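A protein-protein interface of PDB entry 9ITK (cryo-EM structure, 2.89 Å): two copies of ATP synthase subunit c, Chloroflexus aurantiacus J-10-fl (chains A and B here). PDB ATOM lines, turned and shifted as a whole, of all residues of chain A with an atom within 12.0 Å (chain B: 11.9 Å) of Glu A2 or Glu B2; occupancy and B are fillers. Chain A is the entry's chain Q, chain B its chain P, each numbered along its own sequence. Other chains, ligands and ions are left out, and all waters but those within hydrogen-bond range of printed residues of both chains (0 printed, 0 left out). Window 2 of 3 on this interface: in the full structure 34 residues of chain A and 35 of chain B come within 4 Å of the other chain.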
ATOM      1  N   GLU A   2     -22.424 -24.596 -26.990  1.00  0.00           N
ATOM      2  CA  GLU A   2     -21.279 -24.701 -26.095  1.00  0.00           C
ATOM      3  C   GLU A   2     -21.245 -23.538 -25.111  1.00  0.00           C
ATOM      4  O   GLU A   2     -20.241 -23.314 -24.435  1.00  0.00           O
ATOM      5  CB  GLU A   2     -19.975 -24.748 -26.896  1.00  0.00           C
ATOM      6  CG  GLU A   2     -19.663 -23.462 -27.648  1.00  0.00           C
ATOM      7  CD  GLU A   2     -18.427 -23.581 -28.519  1.00  0.00           C
ATOM      8  OE1 GLU A   2     -17.797 -24.658 -28.519  1.00  0.00           O
ATOM      9  OE2 GLU A   2     -18.088 -22.595 -29.208  1.00  0.00           O
ATOM     10  N   GLY A   3     -22.349 -22.802 -25.031  1.00  0.00           N
ATOM     11  CA  GLY A   3     -22.431 -21.628 -24.190  1.00  0.00           C
ATOM     12  C   GLY A   3     -22.085 -20.321 -24.869  1.00  0.00           C
ATOM     13  O   GLY A   3     -21.914 -19.311 -24.176  1.00  0.00           O
ATOM     14  N   LEU A   4     -21.966 -20.306 -26.197  1.00  0.00           N
ATOM     15  CA  LEU A   4     -21.670 -19.072 -26.914  1.00  0.00           C
ATOM     16  C   LEU A   4     -22.825 -18.081 -26.848  1.00  0.00           C
ATOM     17  O   LEU A   4     -22.590 -16.872 -26.760  1.00  0.00           O
ATOM     18  CB  LEU A   4     -21.298 -19.398 -28.365  1.00  0.00           C
ATOM     19  CG  LEU A   4     -20.965 -18.329 -29.410  1.00  0.00           C
ATOM     20  CD1 LEU A   4     -20.223 -18.979 -30.555  1.00  0.00           C
ATOM     21  CD2 LEU A   4     -22.221 -17.688 -29.962  1.00  0.00           C
ATOM     22  N   ASN A   5     -24.069 -18.564 -26.895  1.00  0.00           N
ATOM     23  CA  ASN A   5     -25.211 -17.660 -26.827  1.00  0.00           C
ATOM     24  C   ASN A   5     -25.304 -16.929 -25.494  1.00  0.00           C
ATOM     25  O   ASN A   5     -25.943 -15.875 -25.425  1.00  0.00           O
ATOM     26  CB  ASN A   5     -26.505 -18.426 -27.119  1.00  0.00           C
ATOM     27  CG  ASN A   5     -26.805 -19.500 -26.092  1.00  0.00           C
ATOM     28  OD1 ASN A   5     -26.124 -19.622 -25.078  1.00  0.00           O
ATOM     29  ND2 ASN A   5     -27.840 -20.289 -26.355  1.00  0.00           N
ATOM     30  N   LEU A   6     -24.694 -17.464 -24.434  1.00  0.00           N
ATOM     31  CA  LEU A   6     -24.609 -16.716 -23.185  1.00  0.00           C
ATOM     32  C   LEU A   6     -23.718 -15.490 -23.338  1.00  0.00           C
ATOM     33  O   LEU A   6     -24.011 -14.426 -22.779  1.00  0.00           O
ATOM     34  CB  LEU A   6     -24.096 -17.614 -22.060  1.00  0.00           C
ATOM     35  CG  LEU A   6     -25.153 -18.342 -21.226  1.00  0.00           C
ATOM     36  CD1 LEU A   6     -25.766 -19.499 -21.988  1.00  0.00           C
ATOM     37  CD2 LEU A   6     -24.555 -18.828 -19.923  1.00  0.00           C
ATOM     38  N   VAL A   7     -22.618 -15.621 -24.084  1.00  0.00           N
ATOM     39  CA  VAL A   7     -21.716 -14.491 -24.291  1.00  0.00           C
ATOM     40  C   VAL A   7     -22.416 -13.387 -25.070  1.00  0.00           C
ATOM     41  O   VAL A   7     -22.298 -12.200 -24.740  1.00  0.00           O
ATOM     42  CB  VAL A   7     -20.429 -14.950 -24.998  1.00  0.00           C
ATOM     43  CG1 VAL A   7     -19.551 -13.760 -25.324  1.00  0.00           C
ATOM     44  CG2 VAL A   7     -19.675 -15.936 -24.124  1.00  0.00           C
ATOM     45  N   ALA A   8     -23.157 -13.760 -26.115  1.00  0.00           N
ATOM     46  CA  ALA A   8     -23.845 -12.761 -26.924  1.00  0.00           C
ATOM     47  C   ALA A   8     -24.845 -11.968 -26.092  1.00  0.00           C
ATOM     48  O   ALA A   8     -25.060 -10.776 -26.335  1.00  0.00           O
ATOM     49  CB  ALA A   8     -24.543 -13.429 -28.108  1.00  0.00           C
ATOM     50  N   THR A   9     -25.464 -12.610 -25.101  1.00  0.00           N
ATOM     51  CA  THR A   9     -26.404 -11.899 -24.242  1.00  0.00           C
ATOM     52  C   THR A   9     -25.710 -10.787 -23.465  1.00  0.00           C
ATOM     53  O   THR A   9     -26.236  -9.674 -23.357  1.00  0.00           O
ATOM     54  CB  THR A   9     -27.085 -12.876 -23.286  1.00  0.00           C
ATOM     55  OG1 THR A   9     -27.782 -13.874 -24.041  1.00  0.00           O
ATOM     56  CG2 THR A   9     -28.075 -12.146 -22.399  1.00  0.00           C
ATOM     57  N   ILE A  70     -32.271 -12.894 -27.511  1.00  0.00           N
ATOM     58  CA  ILE A  70     -31.334 -14.005 -27.616  1.00  0.00           C
ATOM     59  C   ILE A  70     -31.420 -14.920 -26.397  1.00  0.00           C
ATOM     60  O   ILE A  70     -31.167 -16.124 -26.507  1.00  0.00           O
ATOM     61  CB  ILE A  70     -29.904 -13.472 -27.814  1.00  0.00           C
ATOM     62  CG1 ILE A  70     -29.844 -12.564 -29.042  1.00  0.00           C
ATOM     63  CG2 ILE A  70     -28.912 -14.613 -27.970  1.00  0.00           C
ATOM     64  CD1 ILE A  70     -30.240 -13.250 -30.327  1.00  0.00           C
ATOM     65  N   GLU B   2     -18.274 -24.869 -22.114  1.00  0.00           N
ATOM     66  CA  GLU B   2     -17.042 -24.781 -21.340  1.00  0.00           C
ATOM     67  C   GLU B   2     -17.180 -23.777 -20.203  1.00  0.00           C
ATOM     68  O   GLU B   2     -18.156 -23.796 -19.454  1.00  0.00           O
ATOM     69  CB  GLU B   2     -15.868 -24.388 -22.238  1.00  0.00           C
ATOM     70  CG  GLU B   2     -15.756 -25.200 -23.514  1.00  0.00           C
ATOM     71  CD  GLU B   2     -16.414 -24.515 -24.693  1.00  0.00           C
ATOM     72  OE1 GLU B   2     -15.712 -24.222 -25.682  1.00  0.00           O
ATOM     73  OE2 GLU B   2     -17.637 -24.272 -24.630  1.00  0.00           O
ATOM     74  N   GLY B   3     -16.188 -22.900 -20.084  1.00  0.00           N
ATOM     75  CA  GLY B   3     -16.206 -21.863 -19.072  1.00  0.00           C
ATOM     76  C   GLY B   3     -16.660 -20.526 -19.615  1.00  0.00           C
ATOM     77  O   GLY B   3     -16.404 -19.483 -19.006  1.00  0.00           O
ATOM     78  N   LEU B   4     -17.331 -20.543 -20.770  1.00  0.00           N
ATOM     79  CA  LEU B   4     -17.814 -19.301 -21.362  1.00  0.00           C
ATOM     80  C   LEU B   4     -18.855 -18.624 -20.482  1.00  0.00           C
ATOM     81  O   LEU B   4     -18.937 -17.391 -20.459  1.00  0.00           O
ATOM     82  CB  LEU B   4     -18.401 -19.565 -22.748  1.00  0.00           C
ATOM     83  CG  LEU B   4     -17.425 -19.557 -23.922  1.00  0.00           C
ATOM     84  CD1 LEU B   4     -18.182 -19.445 -25.234  1.00  0.00           C
ATOM     85  CD2 LEU B   4     -16.422 -18.428 -23.779  1.00  0.00           C
ATOM     86  N   ASN B   5     -19.658 -19.406 -19.759  1.00  0.00           N
ATOM     87  CA  ASN B   5     -20.679 -18.815 -18.900  1.00  0.00           C
ATOM     88  C   ASN B   5     -20.058 -17.967 -17.797  1.00  0.00           C
ATOM     89  O   ASN B   5     -20.613 -16.931 -17.414  1.00  0.00           O
ATOM     90  CB  ASN B   5     -21.598 -19.913 -18.347  1.00  0.00           C
ATOM     91  CG  ASN B   5     -20.930 -20.809 -17.306  1.00  0.00           C
ATOM     92  OD1 ASN B   5     -19.970 -20.431 -16.643  1.00  0.00           O
ATOM     93  ND2 ASN B   5     -21.458 -22.019 -17.163  1.00  0.00           N
ATOM     94  N   LEU B   6     -18.908 -18.389 -17.271  1.00  0.00           N
ATOM     95  CA  LEU B   6     -18.213 -17.570 -16.285  1.00  0.00           C
ATOM     96  C   LEU B   6     -17.605 -16.327 -16.926  1.00  0.00           C
ATOM     97  O   LEU B   6     -17.534 -15.269 -16.292  1.00  0.00           O
ATOM     98  CB  LEU B   6     -17.150 -18.407 -15.572  1.00  0.00           C
ATOM     99  CG  LEU B   6     -17.771 -19.523 -14.725  1.00  0.00           C
ATOM    100  CD1 LEU B   6     -16.737 -20.451 -14.121  1.00  0.00           C
ATOM    101  CD2 LEU B   6     -18.666 -18.943 -13.638  1.00  0.00           C
ATOM    102  N   VAL B   7     -17.155 -16.434 -18.177  1.00  0.00           N
ATOM    103  CA  VAL B   7     -16.662 -15.256 -18.886  1.00  0.00           C
ATOM    104  C   VAL B   7     -17.810 -14.323 -19.243  1.00  0.00           C
ATOM    105  O   VAL B   7     -17.692 -13.099 -19.121  1.00  0.00           O
ATOM    106  CB  VAL B   7     -15.866 -15.673 -20.134  1.00  0.00           C
ATOM    107  CG1 VAL B   7     -15.398 -14.449 -20.895  1.00  0.00           C
ATOM    108  CG2 VAL B   7     -14.681 -16.526 -19.739  1.00  0.00           C
ATOM    109  N   ALA B   8     -18.936 -14.882 -19.690  1.00  0.00           N
ATOM    110  CA  ALA B   8     -20.049 -14.053 -20.138  1.00  0.00           C
ATOM    111  C   ALA B   8     -20.585 -13.187 -19.005  1.00  0.00           C
ATOM    112  O   ALA B   8     -20.844 -11.993 -19.192  1.00  0.00           O
ATOM    113  CB  ALA B   8     -21.158 -14.930 -20.716  1.00  0.00           C
ATOM    114  N   THR B   9     -20.751 -13.768 -17.816  1.00  0.00           N
ATOM    115  CA  THR B   9     -21.238 -12.985 -16.689  1.00  0.00           C
ATOM    116  C   THR B   9     -20.232 -11.933 -16.243  1.00  0.00           C
ATOM    117  O   THR B   9     -20.629 -10.935 -15.633  1.00  0.00           O
ATOM    118  CB  THR B   9     -21.596 -13.897 -15.515  1.00  0.00           C
ATOM    119  OG1 THR B   9     -22.140 -13.110 -14.448  1.00  0.00           O
ATOM    120  CG2 THR B   9     -20.372 -14.632 -15.014  1.00  0.00           C
ATOM    121  N   ILE B  70     -26.923 -14.999 -16.357  1.00  0.00           N
ATOM    122  CA  ILE B  70     -25.964 -15.843 -17.061  1.00  0.00           C
ATOM    123  C   ILE B  70     -25.490 -16.992 -16.183  1.00  0.00           C
ATOM    124  O   ILE B  70     -25.466 -18.149 -16.613  1.00  0.00           O
ATOM    125  CB  ILE B  70     -24.777 -14.992 -17.562  1.00  0.00           C
ATOM    126  CG1 ILE B  70     -25.215 -14.083 -18.711  1.00  0.00           C
ATOM    127  CG2 ILE B  70     -23.630 -15.883 -17.995  1.00  0.00           C
ATOM    128  CD1 ILE B  70     -25.739 -14.830 -19.914  1.00  0.00           C
ATOM    129  N   GLY B  71     -25.108 -16.697 -14.939  1.00  0.00           N
ATOM    130  CA  GLY B  71     -24.626 -17.746 -14.058  1.00  0.00           C
ATOM    131  C   GLY B  71     -25.719 -18.678 -13.574  1.00  0.00           C
ATOM    132  O   GLY B  71     -25.443 -19.823 -13.206  1.00  0.00           O
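The backbone NH (N) of Glu B2 is in hydrogen-bond range of the backbone carbonyl oxygen (O) of Glu A2.
Among the printed residues, merely in contact across the chains: Gly A3 with Leu B4, Leu A4 with Leu B4, Leu A6 with Asn B5, Leu A6 with Ala B8, Leu A6 with Ile B70, Val A7 with Leu B4 and Val A7 with Ala B8.
Glu B2 touches its own counterpart, Glu A2.
Leu A6 touches Asn B5, but with the chains exchanged Asn A5 does not touch Leu B6 (10.5 Å).
Leu A6 touches Ile B70, but with the chains exchanged Ile A70 does not touch Leu B6 (15.1 Å).
Val A7 touches Ala B8, but with the chains exchanged Ala A8 does not touch Val B7 (8.7 Å).
9 positions are printed for both chains.
Of the 8 pairs that touch across the chains among the printed residues, 2 have their exchanged pair printed and touching as well.
Of chain B, only Glu B2 (2.8 Å) comes within 4 Å of Glu A2.
Of chain A, only Glu A2 comes within 4 Å of Glu B2.
Of the printed residues of chain B, Gly A3 touches Leu B4 (3.8 Å).
Of chain B, only Leu B4 comes within 4 Å of Leu A4.
Of chain A, only Gly A3 (3.8 Å), Leu A4 (3.9 Å) and Val A7 (3.97 Å) come within 4 Å of Leu B4.
Asn B5 touches just one residue of chain A: Leu A6.
Of the printed residues of chain A, Ala B8 touches Leu A6 and Val A7.
Printed residues of chain A within 4 Å of Ile B70: Leu A6.
Of the printed residues of chain B, Leu A6 touches Asn B5 (3.5 Å), Ala B8 (3.6 Å) and Ile B70 (3.4 Å).
The nearest residue of chain B that does not touch Glu A2 is Leu B4 (4.5 Å).
The nearest residue of chain A that does not touch Glu B2 is Gly A3 (5.0 Å).
The nearest printed residue of chain B that does not touch Leu A6 is Leu B4 (5.4 Å).
Hydrophobic or aromatic side chains of chain A that line the printed part of chain B: Leu A6 and Val A7.
Along chain A the printed residues that touch a printed residue of chain B span positions 2 to 7.
Among the printed residues, 8 pairs touch across the chains.
Among the printed residues, no Asp or Glu carboxylate lies within 4 Å of a Lys or Arg side-chain nitrogen of the other chain.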
